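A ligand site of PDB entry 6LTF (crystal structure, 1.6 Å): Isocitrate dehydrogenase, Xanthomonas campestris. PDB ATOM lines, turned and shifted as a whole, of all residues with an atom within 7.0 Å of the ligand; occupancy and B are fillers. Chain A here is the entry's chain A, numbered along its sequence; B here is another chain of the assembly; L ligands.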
ATOM      1  N   GLU A 119      -2.074  27.604  13.832  1.00  0.00           N
ATOM      2  CA  GLU A 119      -2.001  26.284  14.472  1.00  0.00           C
ATOM      3  C   GLU A 119      -2.298  26.443  15.969  1.00  0.00           C
ATOM      4  O   GLU A 119      -1.703  27.301  16.614  1.00  0.00           O
ATOM      5  CB  GLU A 119      -0.614  25.675  14.266  1.00  0.00           C
ATOM      6  CG  GLU A 119      -0.569  24.162  14.485  1.00  0.00           C
ATOM      7  CD  GLU A 119      -0.695  23.744  15.940  1.00  0.00           C
ATOM      8  OE1 GLU A 119      -0.142  24.428  16.836  1.00  0.00           O
ATOM      9  OE2 GLU A 119      -1.402  22.749  16.192  1.00  0.00           O
ATOM     10  N   GLU A 122      -0.085  23.031  19.359  1.00  0.00           N
ATOM     11  CA  GLU A 122       1.305  22.871  19.806  1.00  0.00           C
ATOM     12  C   GLU A 122       2.049  24.207  19.727  1.00  0.00           C
ATOM     13  O   GLU A 122       1.469  25.246  20.054  1.00  0.00           O
ATOM     14  CB  GLU A 122       1.997  21.742  19.006  1.00  0.00           C
ATOM     15  CG  GLU A 122       1.929  21.888  17.477  1.00  0.00           C
ATOM     16  CD  GLU A 122       2.539  20.713  16.712  1.00  0.00           C
ATOM     17  OE1 GLU A 122       2.430  19.541  17.181  1.00  0.00           O
ATOM     18  OE2 GLU A 122       3.122  20.958  15.622  1.00  0.00           O
ATOM     19  N   GLY A 123       3.324  24.209  19.340  1.00  0.00           N
ATOM     20  CA  GLY A 123       4.043  25.468  19.303  1.00  0.00           C
ATOM     21  C   GLY A 123       4.453  25.911  20.698  1.00  0.00           C
ATOM     22  O   GLY A 123       4.699  25.102  21.597  1.00  0.00           O
ATOM     23  N   ALA A 124       4.502  27.231  20.901  1.00  0.00           N
ATOM     24  CA  ALA A 124       5.089  27.799  22.125  1.00  0.00           C
ATOM     25  C   ALA A 124       4.095  28.021  23.256  1.00  0.00           C
ATOM     26  O   ALA A 124       4.495  28.553  24.302  1.00  0.00           O
ATOM     27  CB  ALA A 124       5.790  29.114  21.776  1.00  0.00           C
ATOM     28  N   TYR A 125       2.832  27.633  23.103  1.00  0.00           N
ATOM     29  CA  TYR A 125       1.790  27.949  24.071  1.00  0.00           C
ATOM     30  C   TYR A 125       1.340  26.738  24.887  1.00  0.00           C
ATOM     31  O   TYR A 125       0.252  26.742  25.466  1.00  0.00           O
ATOM     32  CB  TYR A 125       0.592  28.590  23.355  1.00  0.00           C
ATOM     33  CG  TYR A 125       0.685  30.093  23.086  1.00  0.00           C
ATOM     34  CD1 TYR A 125       1.814  30.836  23.433  1.00  0.00           C
ATOM     35  CD2 TYR A 125      -0.378  30.752  22.476  1.00  0.00           C
ATOM     36  CE1 TYR A 125       1.884  32.217  23.172  1.00  0.00           C
ATOM     37  CE2 TYR A 125      -0.324  32.118  22.225  1.00  0.00           C
ATOM     38  CZ  TYR A 125       0.792  32.843  22.552  1.00  0.00           C
ATOM     39  OH  TYR A 125       0.805  34.211  22.295  1.00  0.00           O
ATOM     40  N   GLY A 142       8.822  25.836  26.948  1.00  0.00           N
ATOM     41  CA  GLY A 142       9.204  25.051  25.800  1.00  0.00           C
ATOM     42  C   GLY A 142       8.308  25.327  24.608  1.00  0.00           C
ATOM     43  O   GLY A 142       7.269  25.991  24.720  1.00  0.00           O
ATOM     44  N   ALA A 143       8.728  24.798  23.469  1.00  0.00           N
ATOM     45  CA  ALA A 143       7.883  24.742  22.297  1.00  0.00           C
ATOM     46  C   ALA A 143       8.094  23.383  21.645  1.00  0.00           C
ATOM     47  O   ALA A 143       9.207  22.849  21.666  1.00  0.00           O
ATOM     48  CB  ALA A 143       8.198  25.865  21.302  1.00  0.00           C
ATOM     49  N   ARG A 144       7.029  22.831  21.078  1.00  0.00           N
ATOM     50  CA  ARG A 144       7.107  21.593  20.338  1.00  0.00           C
ATOM     51  C   ARG A 144       6.421  21.798  19.001  1.00  0.00           C
ATOM     52  O   ARG A 144       5.295  22.315  18.943  1.00  0.00           O
ATOM     53  CB  ARG A 144       6.450  20.440  21.128  1.00  0.00           C
ATOM     54  CG  ARG A 144       6.694  19.050  20.483  1.00  0.00           C
ATOM     55  CD  ARG A 144       6.045  17.898  21.267  1.00  0.00           C
ATOM     56  NE  ARG A 144       4.661  18.169  21.650  1.00  0.00           N
ATOM     57  CZ  ARG A 144       4.229  18.219  22.911  1.00  0.00           C
ATOM     58  NH1 ARG A 144       5.071  18.005  23.914  1.00  0.00           N
ATOM     59  NH2 ARG A 144       2.942  18.463  23.168  1.00  0.00           N
ATOM     60  N   VAL A 145       7.105  21.428  17.905  1.00  0.00           N
ATOM     61  CA  VAL A 145       6.480  21.430  16.582  1.00  0.00           C
ATOM     62  C   VAL A 145       6.659  20.031  16.018  1.00  0.00           C
ATOM     63  O   VAL A 145       7.755  19.462  16.098  1.00  0.00           O
ATOM     64  CB  VAL A 145       7.085  22.502  15.659  1.00  0.00           C
ATOM     65  CG1 VAL A 145       6.591  22.324  14.224  1.00  0.00           C
ATOM     66  CG2 VAL A 145       6.738  23.892  16.159  1.00  0.00           C
ATOM     67  N   VAL A 172       4.466  31.693   7.513  1.00  0.00           N
ATOM     68  CA  VAL A 172       5.213  32.702   8.282  1.00  0.00           C
ATOM     69  C   VAL A 172       6.034  32.001   9.360  1.00  0.00           C
ATOM     70  O   VAL A 172       5.524  31.121  10.057  1.00  0.00           O
ATOM     71  CB  VAL A 172       4.280  33.764   8.877  1.00  0.00           C
ATOM     72  CG1 VAL A 172       5.056  34.752   9.753  1.00  0.00           C
ATOM     73  CG2 VAL A 172       3.570  34.519   7.752  1.00  0.00           C
ATOM     74  N   HIS A 173       7.308  32.372   9.476  1.00  0.00           N
ATOM     75  CA  HIS A 173       8.234  31.569  10.278  1.00  0.00           C
ATOM     76  C   HIS A 173       9.392  32.415  10.813  1.00  0.00           C
ATOM     77  O   HIS A 173       9.539  33.592  10.467  1.00  0.00           O
ATOM     78  CB  HIS A 173       8.816  30.441   9.427  1.00  0.00           C
ATOM     79  CG  HIS A 173       9.670  30.962   8.314  1.00  0.00           C
ATOM     80  ND1 HIS A 173      11.027  31.192   8.463  1.00  0.00           N
ATOM     81  CD2 HIS A 173       9.355  31.349   7.051  1.00  0.00           C
ATOM     82  CE1 HIS A 173      11.513  31.680   7.330  1.00  0.00           C
ATOM     83  NE2 HIS A 173      10.518  31.787   6.466  1.00  0.00           N
ATOM     84  N   LYS A 174      10.216  31.795  11.646  1.00  0.00           N
ATOM     85  CA  LYS A 174      11.497  32.355  12.067  1.00  0.00           C
ATOM     86  C   LYS A 174      12.573  31.275  12.016  1.00  0.00           C
ATOM     87  O   LYS A 174      13.341  31.055  12.966  1.00  0.00           O
ATOM     88  CB  LYS A 174      11.396  32.994  13.456  1.00  0.00           C
ATOM     89  CG  LYS A 174      12.586  33.854  13.882  1.00  0.00           C
ATOM     90  CD  LYS A 174      12.527  35.275  13.289  1.00  0.00           C
ATOM     91  CE  LYS A 174      13.787  36.063  13.600  1.00  0.00           C
ATOM     92  NZ  LYS A 174      13.685  37.477  13.118  1.00  0.00           N
ATOM     93  N   ILE A 178      15.185  30.160  15.078  1.00  0.00           N
ATOM     94  CA  ILE A 178      14.649  28.988  15.777  1.00  0.00           C
ATOM     95  C   ILE A 178      14.605  27.877  14.740  1.00  0.00           C
ATOM     96  O   ILE A 178      13.580  27.581  14.119  1.00  0.00           O
ATOM     97  CB  ILE A 178      13.276  29.252  16.432  1.00  0.00           C
ATOM     98  CG1 ILE A 178      13.257  30.604  17.164  1.00  0.00           C
ATOM     99  CG2 ILE A 178      12.928  28.133  17.399  1.00  0.00           C
ATOM    100  CD1 ILE A 178      11.926  30.878  17.844  1.00  0.00           C
ATOM    101  N   SER A 180      15.134  24.506  14.792  1.00  0.00           N
ATOM    102  CA  SER A 180      14.509  23.199  15.008  1.00  0.00           C
ATOM    103  C   SER A 180      12.997  23.265  14.759  1.00  0.00           C
ATOM    104  O   SER A 180      12.502  22.644  13.813  1.00  0.00           O
ATOM    105  CB  SER A 180      14.798  22.694  16.413  1.00  0.00           C
ATOM    106  OG  SER A 180      14.373  23.637  17.396  1.00  0.00           O
ATOM    107  N   THR A 181      12.265  24.020  15.586  1.00  0.00           N
ATOM    108  CA  THR A 181      10.790  24.006  15.553  1.00  0.00           C
ATOM    109  C   THR A 181      10.227  24.796  14.363  1.00  0.00           C
ATOM    110  O   THR A 181       9.437  24.255  13.563  1.00  0.00           O
ATOM    111  CB  THR A 181      10.254  24.566  16.860  1.00  0.00           C
ATOM    112  OG1 THR A 181      11.024  25.728  17.229  1.00  0.00           O
ATOM    113  CG2 THR A 181      10.337  23.509  17.989  1.00  0.00           C
ATOM    114  N   SER A 182      10.571  26.087  14.251  1.00  0.00           N
ATOM    115  CA  SER A 182      10.078  26.874  13.124  1.00  0.00           C
ATOM    116  C   SER A 182      10.639  26.360  11.788  1.00  0.00           C
ATOM    117  O   SER A 182       9.940  26.389  10.760  1.00  0.00           O
ATOM    118  CB  SER A 182      10.412  28.352  13.328  1.00  0.00           C
ATOM    119  OG  SER A 182       9.611  29.157  12.444  1.00  0.00           O
ATOM    120  N   GLY A 183      11.865  25.810  11.812  1.00  0.00           N
ATOM    121  CA  GLY A 183      12.430  25.228  10.614  1.00  0.00           C
ATOM    122  C   GLY A 183      11.678  23.985  10.158  1.00  0.00           C
ATOM    123  O   GLY A 183      11.471  23.784   8.950  1.00  0.00           O
ATOM    124  N   THR A 225       0.536  29.863   9.960  1.00  0.00           N
ATOM    125  CA  THR A 225       1.674  29.961  10.873  1.00  0.00           C
ATOM    126  C   THR A 225       1.393  29.184  12.159  1.00  0.00           C
ATOM    127  O   THR A 225       0.317  28.604  12.352  1.00  0.00           O
ATOM    128  CB  THR A 225       2.013  31.434  11.170  1.00  0.00           C
ATOM    129  OG1 THR A 225       3.335  31.545  11.741  1.00  0.00           O
ATOM    130  CG2 THR A 225       0.984  32.056  12.086  1.00  0.00           C
ATOM    131  N   THR A 226       2.417  29.172  13.006  1.00  0.00           N
ATOM    132  CA  THR A 226       2.427  28.456  14.275  1.00  0.00           C
ATOM    133  C   THR A 226       1.665  29.252  15.340  1.00  0.00           C
ATOM    134  O   THR A 226       1.183  30.370  15.106  1.00  0.00           O
ATOM    135  CB  THR A 226       3.870  28.157  14.680  1.00  0.00           C
ATOM    136  OG1 THR A 226       4.680  29.319  14.449  1.00  0.00           O
ATOM    137  CG2 THR A 226       4.447  26.961  13.866  1.00  0.00           C
ATOM    138  N   ASN A 227       1.554  28.661  16.538  1.00  0.00           N
ATOM    139  CA  ASN A 227       0.543  29.083  17.509  1.00  0.00           C
ATOM    140  C   ASN A 227       0.748  30.529  17.978  1.00  0.00           C
ATOM    141  O   ASN A 227      -0.143  31.394  17.836  1.00  0.00           O
ATOM    142  CB  ASN A 227       0.549  28.073  18.674  1.00  0.00           C
ATOM    143  CG  ASN A 227      -0.741  28.091  19.507  1.00  0.00           C
ATOM    144  OD1 ASN A 227      -1.539  29.031  19.432  1.00  0.00           O
ATOM    145  ND2 ASN A 227      -0.930  27.041  20.307  1.00  0.00           N
ATOM    146  N   LEU A 228       1.898  30.805  18.566  1.00  0.00           N
ATOM    147  CA  LEU A 228       2.183  32.141  19.101  1.00  0.00           C
ATOM    148  C   LEU A 228       2.178  33.200  17.994  1.00  0.00           C
ATOM    149  O   LEU A 228       1.551  34.273  18.123  1.00  0.00           O
ATOM    150  CB  LEU A 228       3.525  32.091  19.854  1.00  0.00           C
ATOM    151  CG  LEU A 228       4.192  33.321  20.484  1.00  0.00           C
ATOM    152  CD1 LEU A 228       5.312  32.895  21.474  1.00  0.00           C
ATOM    153  CD2 LEU A 228       4.761  34.280  19.447  1.00  0.00           C
ATOM    154  N   PHE A 229       2.868  32.911  16.880  1.00  0.00           N
ATOM    155  CA  PHE A 229       2.909  33.843  15.757  1.00  0.00           C
ATOM    156  C   PHE A 229       1.493  34.146  15.253  1.00  0.00           C
ATOM    157  O   PHE A 229       1.190  35.292  14.893  1.00  0.00           O
ATOM    158  CB  PHE A 229       3.761  33.294  14.584  1.00  0.00           C
ATOM    159  CG  PHE A 229       5.244  33.233  14.863  1.00  0.00           C
ATOM    160  CD1 PHE A 229       5.835  33.900  15.931  1.00  0.00           C
ATOM    161  CD2 PHE A 229       6.067  32.496  13.991  1.00  0.00           C
ATOM    162  CE1 PHE A 229       7.228  33.822  16.132  1.00  0.00           C
ATOM    163  CE2 PHE A 229       7.443  32.403  14.202  1.00  0.00           C
ATOM    164  CZ  PHE A 229       8.022  33.077  15.272  1.00  0.00           C
ATOM    165  N   GLY A 230       0.623  33.130  15.206  1.00  0.00           N
ATOM    166  CA  GLY A 230      -0.741  33.338  14.713  1.00  0.00           C
ATOM    167  C   GLY A 230      -1.594  34.167  15.655  1.00  0.00           C
ATOM    168  O   GLY A 230      -2.390  34.998  15.211  1.00  0.00           O
ATOM    169  N   ASP A 231      -1.439  33.947  16.970  1.00  0.00           N
ATOM    170  CA  ASP A 231      -2.053  34.822  17.957  1.00  0.00           C
ATOM    171  C   ASP A 231      -1.753  36.290  17.648  1.00  0.00           C
ATOM    172  O   ASP A 231      -2.669  37.132  17.468  1.00  0.00           O
ATOM    173  CB  ASP A 231      -1.509  34.429  19.334  1.00  0.00           C
ATOM    174  CG  ASP A 231      -2.190  35.143  20.470  1.00  0.00           C
ATOM    175  OD1 ASP A 231      -3.385  35.486  20.331  1.00  0.00           O
ATOM    176  OD2 ASP A 231      -1.523  35.348  21.511  1.00  0.00           O
ATOM    177  N   ALA B 124      13.242  33.429  23.826  1.00  0.00           N
ATOM    178  CA  ALA B 124      12.946  32.286  22.967  1.00  0.00           C
ATOM    179  C   ALA B 124      13.919  32.105  21.795  1.00  0.00           C
ATOM    180  O   ALA B 124      13.701  31.197  20.984  1.00  0.00           O
ATOM    181  CB  ALA B 124      11.518  32.409  22.428  1.00  0.00           C
ATOM    182  N   TYR B 125      14.968  32.917  21.691  1.00  0.00           N
ATOM    183  CA  TYR B 125      15.851  32.915  20.532  1.00  0.00           C
ATOM    184  C   TYR B 125      17.222  32.306  20.821  1.00  0.00           C
ATOM    185  O   TYR B 125      18.188  32.559  20.097  1.00  0.00           O
ATOM    186  CB  TYR B 125      16.001  34.346  19.992  1.00  0.00           C
ATOM    187  CG  TYR B 125      14.896  34.841  19.063  1.00  0.00           C
ATOM    188  CD1 TYR B 125      13.787  34.045  18.738  1.00  0.00           C
ATOM    189  CD2 TYR B 125      14.977  36.106  18.496  1.00  0.00           C
ATOM    190  CE1 TYR B 125      12.788  34.516  17.870  1.00  0.00           C
ATOM    191  CE2 TYR B 125      14.003  36.576  17.627  1.00  0.00           C
ATOM    192  CZ  TYR B 125      12.911  35.804  17.328  1.00  0.00           C
ATOM    193  OH  TYR B 125      11.949  36.310  16.464  1.00  0.00           O
ATOM    194  N   SER B 141      12.188  23.370  20.963  1.00  0.00           N
ATOM    195  CA  SER B 141      13.006  24.543  21.246  1.00  0.00           C
ATOM    196  C   SER B 141      12.600  25.033  22.624  1.00  0.00           C
ATOM    197  O   SER B 141      11.588  24.618  23.182  1.00  0.00           O
ATOM    198  CB  SER B 141      12.867  25.623  20.161  1.00  0.00           C
ATOM    199  OG  SER B 141      11.540  26.114  20.060  1.00  0.00           O
ATOM    200  N   LEU B 228      11.908  37.622  21.453  1.00  0.00           N
ATOM    201  CA  LEU B 228      11.091  37.354  20.265  1.00  0.00           C
ATOM    202  C   LEU B 228      10.013  38.435  20.088  1.00  0.00           C
ATOM    203  O   LEU B 228       9.825  38.972  18.966  1.00  0.00           O
ATOM    204  CB  LEU B 228      10.480  35.944  20.403  1.00  0.00           C
ATOM    205  CG  LEU B 228       9.503  35.342  19.387  1.00  0.00           C
ATOM    206  CD1 LEU B 228       9.380  33.812  19.593  1.00  0.00           C
ATOM    207  CD2 LEU B 228       8.116  35.983  19.457  1.00  0.00           C
HETATM  208  C1  LIG L   1       4.850  29.540  17.779  1.00  0.00           C
HETATM  209  O1  LIG L   1       4.160  28.943  18.631  1.00  0.00           O
HETATM  210  O2  LIG L   1       4.393  30.347  16.928  1.00  0.00           O
HETATM  211  C2  LIG L   1       6.324  29.287  17.835  1.00  0.00           C
HETATM  212  C3  LIG L   1       6.610  27.816  17.965  1.00  0.00           C
HETATM  213  C4  LIG L   1       8.094  27.488  17.993  1.00  0.00           C
HETATM  214  C5  LIG L   1       8.945  28.251  16.988  1.00  0.00           C
HETATM  215  C6  LIG L   1       8.477  29.676  16.701  1.00  0.00           C
HETATM  216  C7  LIG L   1       6.985  29.862  16.613  1.00  0.00           C
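The side-chain hydroxyl (OG1) of Thr 181 sits at hydrogen-bond distance from the side-chain hydroxyl (OG) of Ser 141 of chain B. The side-chain amide nitrogen (ND2) of Asn 227 is in hydrogen-bond range of the backbone carbonyl oxygen (O) of Glu 122 (3.0 Å). The backbone carbonyl oxygen (O) of Glu 119 lies close to the side-chain amide oxygen (OD1) of Asn 227, 3.3 Å away. The backbone carbonyl oxygen of Arg 144 lies within hydrogen-bond range of the backbone NH of Gly 123 (2.8 Å). The backbone carbonyl oxygen of Ser 141 of chain B is in hydrogen-bond range of the backbone NH of Ala 143. The backbone carbonyl oxygen of Ile 178 sits at hydrogen-bond distance from the backbone NH of Gly 183 (3.4 Å). The backbone NH of Lys 174 sits at hydrogen-bond distance from the side-chain hydroxyl of Ser 182, 2.8 Å away.
The side-chain hydroxyl (OG1) of Thr 226 sits at hydrogen-bond distance from an oxygen (O2) of the ligand (2.7 Å). The backbone NH of Ala 124 of chain A lies within hydrogen-bond range of an oxygen (O1) of the ligand (2.9 Å). The backbone NH (N) of Leu 228 of chain A is in hydrogen-bond range of an oxygen (O1) of the ligand, at 2.9 Å. The backbone NH (N) of Phe 229 sits at hydrogen-bond distance from an oxygen (O2) of the ligand. The backbone NH of Asn 227 is in hydrogen-bond range of an oxygen (O2) of the ligand, 3.3 Å away.
Merely in contact with the ligand: Thr 181, Gly 123, Ala 143, Ile 178 and Ser 182. Within 4 Å of the ligand: Gly 123, Ala 124 of chain A, Ala 143, Ile 178, Thr 181, Ser 182, Thr 226, Asn 227, Leu 228 of chain A and Phe 229.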
